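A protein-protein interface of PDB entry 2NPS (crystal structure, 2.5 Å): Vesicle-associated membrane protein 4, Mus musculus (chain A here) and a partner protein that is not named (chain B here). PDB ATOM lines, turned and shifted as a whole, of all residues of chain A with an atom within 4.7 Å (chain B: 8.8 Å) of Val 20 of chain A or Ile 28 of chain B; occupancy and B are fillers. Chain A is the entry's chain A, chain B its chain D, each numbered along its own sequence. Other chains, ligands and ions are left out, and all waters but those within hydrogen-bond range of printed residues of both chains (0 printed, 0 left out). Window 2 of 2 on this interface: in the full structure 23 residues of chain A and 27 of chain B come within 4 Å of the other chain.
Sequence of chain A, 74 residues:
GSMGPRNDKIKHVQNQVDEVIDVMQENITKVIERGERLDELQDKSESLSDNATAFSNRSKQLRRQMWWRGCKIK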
ATOM      1  N   GLN A  16     -16.822  25.879 -27.092  1.00  0.00           N
ATOM      2  CA  GLN A  16     -16.110  24.751 -27.653  1.00  0.00           C
ATOM      3  C   GLN A  16     -14.670  25.083 -27.261  1.00  0.00           C
ATOM      4  O   GLN A  16     -13.877  24.221 -26.897  1.00  0.00           O
ATOM      5  CB  GLN A  16     -16.245  24.802 -29.160  1.00  0.00           C
ATOM      6  CG  GLN A  16     -16.751  23.568 -29.810  1.00  0.00           C
ATOM      7  CD  GLN A  16     -16.213  23.459 -31.203  1.00  0.00           C
ATOM      8  OE1 GLN A  16     -16.817  23.932 -32.170  1.00  0.00           O
ATOM      9  NE2 GLN A  16     -15.044  22.850 -31.317  1.00  0.00           N
ATOM     10  N   VAL A  17     -14.374  26.376 -27.361  1.00  0.00           N
ATOM     11  CA  VAL A  17     -13.085  26.978 -27.031  1.00  0.00           C
ATOM     12  C   VAL A  17     -12.933  26.949 -25.536  1.00  0.00           C
ATOM     13  O   VAL A  17     -11.898  26.565 -25.015  1.00  0.00           O
ATOM     14  CB  VAL A  17     -13.029  28.477 -27.458  1.00  0.00           C
ATOM     15  N   ASP A  18     -13.986  27.387 -24.861  1.00  0.00           N
ATOM     16  CA  ASP A  18     -13.992  27.440 -23.412  1.00  0.00           C
ATOM     17  C   ASP A  18     -13.745  26.049 -22.882  1.00  0.00           C
ATOM     18  O   ASP A  18     -13.257  25.886 -21.766  1.00  0.00           O
ATOM     19  CB  ASP A  18     -15.331  27.956 -22.889  1.00  0.00           C
ATOM     20  CG  ASP A  18     -15.558  29.431 -23.199  1.00  0.00           C
ATOM     21  OD1 ASP A  18     -16.676  29.927 -22.937  1.00  0.00           O
ATOM     22  OD2 ASP A  18     -14.625  30.102 -23.702  1.00  0.00           O
ATOM     23  N   GLU A  19     -14.082  25.047 -23.691  1.00  0.00           N
ATOM     24  CA  GLU A  19     -13.862  23.663 -23.296  1.00  0.00           C
ATOM     25  C   GLU A  19     -12.365  23.394 -23.391  1.00  0.00           C
ATOM     26  O   GLU A  19     -11.747  22.919 -22.438  1.00  0.00           O
ATOM     27  CB  GLU A  19     -14.620  22.708 -24.217  1.00  0.00           C
ATOM     28  N   VAL A  20     -11.785  23.698 -24.549  1.00  0.00           N
ATOM     29  CA  VAL A  20     -10.351  23.500 -24.726  1.00  0.00           C
ATOM     30  C   VAL A  20      -9.607  24.240 -23.616  1.00  0.00           C
ATOM     31  O   VAL A  20      -8.634  23.733 -23.065  1.00  0.00           O
ATOM     32  CB  VAL A  20      -9.857  24.016 -26.097  1.00  0.00           C
ATOM     33  CG1 VAL A  20      -8.371  23.754 -26.242  1.00  0.00           C
ATOM     34  CG2 VAL A  20     -10.605  23.329 -27.216  1.00  0.00           C
ATOM     35  N   ILE A  21     -10.083  25.436 -23.285  1.00  0.00           N
ATOM     36  CA  ILE A  21      -9.469  26.226 -22.226  1.00  0.00           C
ATOM     37  C   ILE A  21      -9.581  25.466 -20.912  1.00  0.00           C
ATOM     38  O   ILE A  21      -8.692  25.538 -20.070  1.00  0.00           O
ATOM     39  CB  ILE A  21     -10.156  27.597 -22.043  1.00  0.00           C
ATOM     40  CG1 ILE A  21      -9.975  28.460 -23.295  1.00  0.00           C
ATOM     41  CG2 ILE A  21      -9.563  28.314 -20.834  1.00  0.00           C
ATOM     42  N   ASP A  22     -10.679  24.738 -20.743  1.00  0.00           N
ATOM     43  CA  ASP A  22     -10.909  23.968 -19.529  1.00  0.00           C
ATOM     44  C   ASP A  22      -9.950  22.793 -19.414  1.00  0.00           C
ATOM     45  O   ASP A  22      -9.459  22.490 -18.332  1.00  0.00           O
ATOM     46  CB  ASP A  22     -12.339  23.451 -19.506  1.00  0.00           C
ATOM     47  CG  ASP A  22     -12.566  22.421 -18.410  1.00  0.00           C
ATOM     48  OD1 ASP A  22     -12.518  22.809 -17.212  1.00  0.00           O
ATOM     49  OD2 ASP A  22     -12.784  21.224 -18.749  1.00  0.00           O
ATOM     50  N   VAL A  23      -9.698  22.134 -20.538  1.00  0.00           N
ATOM     51  CA  VAL A  23      -8.792  20.993 -20.580  1.00  0.00           C
ATOM     52  C   VAL A  23      -7.349  21.453 -20.359  1.00  0.00           C
ATOM     53  O   VAL A  23      -6.604  20.879 -19.568  1.00  0.00           O
ATOM     54  CB  VAL A  23      -8.881  20.298 -21.936  1.00  0.00           C
ATOM     55  CG1 VAL A  23      -8.035  19.042 -21.937  1.00  0.00           C
ATOM     56  CG2 VAL A  23     -10.320  19.978 -22.256  1.00  0.00           C
ATOM     57  N   MET A  24      -6.963  22.498 -21.079  1.00  0.00           N
ATOM     58  CA  MET A  24      -5.614  23.037 -20.977  1.00  0.00           C
ATOM     59  C   MET A  24      -5.318  23.537 -19.573  1.00  0.00           C
ATOM     60  O   MET A  24      -4.224  23.327 -19.047  1.00  0.00           O
ATOM     61  CB  MET A  24      -5.422  24.172 -21.983  1.00  0.00           C
ATOM     62  CG  MET A  24      -5.298  23.693 -23.409  1.00  0.00           C
ATOM     63  SD  MET A  24      -4.034  22.408 -23.529  1.00  0.00           S
ATOM     64  CE  MET A  24      -2.556  23.373 -23.745  1.00  0.00           C
ATOM     65  N   LEU B  21     -16.683  29.975 -39.987  1.00  0.00           N
ATOM     66  CA  LEU B  21     -16.828  29.632 -38.580  1.00  0.00           C
ATOM     67  C   LEU B  21     -16.808  28.113 -38.492  1.00  0.00           C
ATOM     68  O   LEU B  21     -16.674  27.521 -37.421  1.00  0.00           O
ATOM     69  CB  LEU B  21     -18.160  30.163 -38.036  1.00  0.00           C
ATOM     70  CG  LEU B  21     -18.086  31.350 -37.082  1.00  0.00           C
ATOM     71  N   GLU B  22     -16.975  27.495 -39.650  1.00  0.00           N
ATOM     72  CA  GLU B  22     -16.958  26.050 -39.774  1.00  0.00           C
ATOM     73  C   GLU B  22     -15.478  25.685 -39.753  1.00  0.00           C
ATOM     74  O   GLU B  22     -15.081  24.718 -39.115  1.00  0.00           O
ATOM     75  CB  GLU B  22     -17.612  25.638 -41.101  1.00  0.00           C
ATOM     76  CG  GLU B  22     -17.917  24.155 -41.265  1.00  0.00           C
ATOM     77  CD  GLU B  22     -18.890  23.633 -40.219  1.00  0.00           C
ATOM     78  OE1 GLU B  22     -19.852  24.370 -39.894  1.00  0.00           O
ATOM     79  OE2 GLU B  22     -18.702  22.484 -39.738  1.00  0.00           O
ATOM     80  N   LEU B  23     -14.671  26.488 -40.447  1.00  0.00           N
ATOM     81  CA  LEU B  23     -13.216  26.303 -40.516  1.00  0.00           C
ATOM     82  C   LEU B  23     -12.578  26.529 -39.141  1.00  0.00           C
ATOM     83  O   LEU B  23     -11.555  25.937 -38.805  1.00  0.00           O
ATOM     84  CB  LEU B  23     -12.595  27.278 -41.532  1.00  0.00           C
ATOM     85  CG  LEU B  23     -12.801  27.042 -43.029  1.00  0.00           C
ATOM     86  N   VAL B  24     -13.197  27.404 -38.357  1.00  0.00           N
ATOM     87  CA  VAL B  24     -12.710  27.697 -37.016  1.00  0.00           C
ATOM     88  C   VAL B  24     -13.125  26.549 -36.118  1.00  0.00           C
ATOM     89  O   VAL B  24     -12.326  26.047 -35.329  1.00  0.00           O
ATOM     90  CB  VAL B  24     -13.294  29.019 -36.464  1.00  0.00           C
ATOM     91  CG1 VAL B  24     -13.244  29.023 -34.952  1.00  0.00           C
ATOM     92  CG2 VAL B  24     -12.508  30.212 -37.015  1.00  0.00           C
ATOM     93  N   SER B  25     -14.373  26.120 -36.257  1.00  0.00           N
ATOM     94  CA  SER B  25     -14.894  25.023 -35.452  1.00  0.00           C
ATOM     95  C   SER B  25     -14.135  23.736 -35.680  1.00  0.00           C
ATOM     96  O   SER B  25     -13.981  22.921 -34.769  1.00  0.00           O
ATOM     97  CB  SER B  25     -16.359  24.769 -35.767  1.00  0.00           C
ATOM     98  OG  SER B  25     -16.756  23.520 -35.226  1.00  0.00           O
ATOM     99  N   GLY B  26     -13.674  23.542 -36.907  1.00  0.00           N
ATOM    100  CA  GLY B  26     -12.928  22.339 -37.200  1.00  0.00           C
ATOM    101  C   GLY B  26     -11.587  22.478 -36.515  1.00  0.00           C
ATOM    102  O   GLY B  26     -11.194  21.643 -35.700  1.00  0.00           O
ATOM    103  N   SER B  27     -10.891  23.559 -36.847  1.00  0.00           N
ATOM    104  CA  SER B  27      -9.579  23.833 -36.285  1.00  0.00           C
ATOM    105  C   SER B  27      -9.560  23.660 -34.780  1.00  0.00           C
ATOM    106  O   SER B  27      -8.676  23.005 -34.236  1.00  0.00           O
ATOM    107  CB  SER B  27      -9.138  25.256 -36.630  1.00  0.00           C
ATOM    108  OG  SER B  27      -7.930  25.589 -35.954  1.00  0.00           O
ATOM    109  N   ILE B  28     -10.541  24.255 -34.112  1.00  0.00           N
ATOM    110  CA  ILE B  28     -10.624  24.171 -32.665  1.00  0.00           C
ATOM    111  C   ILE B  28     -10.864  22.748 -32.195  1.00  0.00           C
ATOM    112  O   ILE B  28     -10.258  22.299 -31.225  1.00  0.00           O
ATOM    113  CB  ILE B  28     -11.740  25.049 -32.112  1.00  0.00           C
ATOM    114  CG1 ILE B  28     -11.873  24.820 -30.612  1.00  0.00           C
ATOM    115  CG2 ILE B  28     -13.042  24.704 -32.777  1.00  0.00           C
ATOM    116  N   GLY B  29     -11.760  22.045 -32.880  1.00  0.00           N
ATOM    117  CA  GLY B  29     -12.061  20.675 -32.516  1.00  0.00           C
ATOM    118  C   GLY B  29     -10.779  19.900 -32.300  1.00  0.00           C
ATOM    119  O   GLY B  29     -10.622  19.199 -31.301  1.00  0.00           O
ATOM    120  N   VAL B  30      -9.860  20.035 -33.253  1.00  0.00           N
ATOM    121  CA  VAL B  30      -8.564  19.364 -33.189  1.00  0.00           C
ATOM    122  C   VAL B  30      -7.831  19.784 -31.915  1.00  0.00           C
ATOM    123  O   VAL B  30      -7.285  18.947 -31.188  1.00  0.00           O
ATOM    124  CB  VAL B  30      -7.686  19.724 -34.405  1.00  0.00           C
ATOM    125  CG1 VAL B  30      -6.289  19.138 -34.243  1.00  0.00           C
ATOM    126  CG2 VAL B  30      -8.331  19.199 -35.671  1.00  0.00           C
ATOM    127  N   LEU B  31      -7.819  21.087 -31.648  1.00  0.00           N
ATOM    128  CA  LEU B  31      -7.172  21.611 -30.453  1.00  0.00           C
ATOM    129  C   LEU B  31      -7.819  20.921 -29.270  1.00  0.00           C
ATOM    130  O   LEU B  31      -7.154  20.574 -28.298  1.00  0.00           O
ATOM    131  CB  LEU B  31      -7.384  23.123 -30.340  1.00  0.00           C
ATOM    132  CG  LEU B  31      -6.735  23.982 -31.421  1.00  0.00           C
ATOM    133  N   LYS B  32      -9.130  20.726 -29.367  1.00  0.00           N
ATOM    134  CA  LYS B  32      -9.887  20.053 -28.321  1.00  0.00           C
ATOM    135  C   LYS B  32      -9.451  18.598 -28.269  1.00  0.00           C
ATOM    136  O   LYS B  32      -9.613  17.929 -27.255  1.00  0.00           O
ATOM    137  CB  LYS B  32     -11.385  20.123 -28.612  1.00  0.00           C
ATOM    138  CG  LYS B  32     -12.226  19.282 -27.672  1.00  0.00           C
ATOM    139  N   ASN B  33      -8.909  18.109 -29.379  1.00  0.00           N
ATOM    140  CA  ASN B  33      -8.438  16.733 -29.444  1.00  0.00           C
ATOM    141  C   ASN B  33      -7.053  16.663 -28.857  1.00  0.00           C
ATOM    142  O   ASN B  33      -6.779  15.837 -27.990  1.00  0.00           O
ATOM    143  CB  ASN B  33      -8.376  16.230 -30.888  1.00  0.00           C
ATOM    144  CG  ASN B  33      -7.716  14.866 -30.998  1.00  0.00           C
ATOM    145  OD1 ASN B  33      -6.561  14.746 -31.428  1.00  0.00           O
ATOM    146  ND2 ASN B  33      -8.448  13.828 -30.597  1.00  0.00           N
ATOM    147  N   MET B  34      -6.180  17.533 -29.345  1.00  0.00           N
ATOM    148  CA  MET B  34      -4.803  17.566 -28.891  1.00  0.00           C
ATOM    149  C   MET B  34      -4.690  17.856 -27.413  1.00  0.00           C
ATOM    150  O   MET B  34      -3.837  17.300 -26.742  1.00  0.00           O
ATOM    151  CB  MET B  34      -4.005  18.611 -29.670  1.00  0.00           C
ATOM    152  CG  MET B  34      -3.666  18.224 -31.097  1.00  0.00           C
ATOM    153  SD  MET B  34      -2.703  19.525 -31.933  1.00  0.00           S
ATOM    154  CE  MET B  34      -2.670  18.892 -33.585  1.00  0.00           C
ATOM    155  N   SER B  35      -5.547  18.726 -26.897  1.00  0.00           N
ATOM    156  CA  SER B  35      -5.469  19.047 -25.486  1.00  0.00           C
ATOM    157  C   SER B  35      -5.743  17.817 -24.629  1.00  0.00           C
ATOM    158  O   SER B  35      -5.068  17.589 -23.631  1.00  0.00           O
ATOM    159  CB  SER B  35      -6.441  20.177 -25.124  1.00  0.00           C
ATOM    160  OG  SER B  35      -7.786  19.771 -25.248  1.00  0.00           O
ATOM    161  N   GLN B  36      -6.712  17.003 -25.027  1.00  0.00           N
ATOM    162  CA  GLN B  36      -7.046  15.806 -24.256  1.00  0.00           C
ATOM    163  C   GLN B  36      -5.987  14.712 -24.297  1.00  0.00           C
ATOM    164  O   GLN B  36      -5.680  14.105 -23.277  1.00  0.00           O
ATOM    165  CB  GLN B  36      -8.382  15.236 -24.718  1.00  0.00           C
ATOM    166  CG  GLN B  36      -9.505  16.236 -24.698  1.00  0.00           C
ATOM    167  CD  GLN B  36     -10.838  15.586 -24.935  1.00  0.00           C
ATOM    168  OE1 GLN B  36     -11.335  14.845 -24.081  1.00  0.00           O
ATOM    169  NE2 GLN B  36     -11.431  15.846 -26.101  1.00  0.00           N
ATOM    170  N   ILE B  38      -3.031  15.153 -24.557  1.00  0.00           N
ATOM    171  CA  ILE B  38      -1.969  15.750 -23.757  1.00  0.00           C
ATOM    172  C   ILE B  38      -2.254  15.487 -22.295  1.00  0.00           C
ATOM    173  O   ILE B  38      -1.359  15.135 -21.532  1.00  0.00           O
ATOM    174  CB  ILE B  38      -1.914  17.277 -23.969  1.00  0.00           C
ATOM    175  CG1 ILE B  38      -1.424  17.587 -25.385  1.00  0.00           C
ATOM    176  CG2 ILE B  38      -1.030  17.923 -22.911  1.00  0.00           C
ATOM    177  CD1 ILE B  38      -1.588  19.041 -25.783  1.00  0.00           C
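The backbone carbonyl oxygen (O) of Leu 31 of chain B lies within hydrogen-bond range of the side-chain hydroxyl (OG) of Ser 35 of chain B.
O of Lys 32 of chain B lies within hydrogen-bond range of OG of Ser 35 of chain B, at 3.3 Å.
O of Lys 32 of chain B lies within hydrogen-bond range of NE2 of Gln 36 of chain B (3.0 Å).
Ile 28 of chain B touches Gln 16 of chain A.
Gly 29 of chain B touches Gln 16 of chain A (N to NE2, 3.7 Å).
Ile 28 of chain B touches Val 20 of chain A.
Val 20 of chain A touches Leu 31 of chain B (CG1 to O, 3.98 Å).
CG2 of Val 20 of chain A touches CA of Lys 32 of chain B, 3.5 Å away.
Ser 35 of chain B touches Val 23 of chain A.
Gln 36 of chain B touches Val 23 of chain A.
Met 24 of chain A touches Ser 35 of chain B (SD to CB, 3.6 Å).
Hydrophobic or aromatic side chains of chain B within 4 Å of the printed part of chain A: Ile 28.
Of the 9 printed residues of chain A, 4 touch a printed residue of chain B.
Hydrophobic or aromatic side chains of chain A that line the printed part of chain B: Val 20, Val 23 and Met 24.
The side-chain hydroxyl of Ser 25 of chain B sits at hydrogen-bond distance from the side-chain amide oxygen of Gln 16 of chain A.
Of the printed residues of chain B, Val 20 of chain A touches Ile 28, Leu 31 and Lys 32.
Of chain A, only Gln 16 and Val 20 come within 4 Å of Ile 28 of chain B.
Of the printed residues of chain A, Gly 29 of chain B touches Gln 16.
Of the printed residues of chain B, Met 24 of chain A touches Ser 35 (3.6 Å).
Of the printed residues of chain A, Leu 31 of chain B touches Val 20 (3.98 Å).
The nearest residue of chain A that does not touch Ile 28 of chain B is Val 17 of chain A (4.4 Å).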
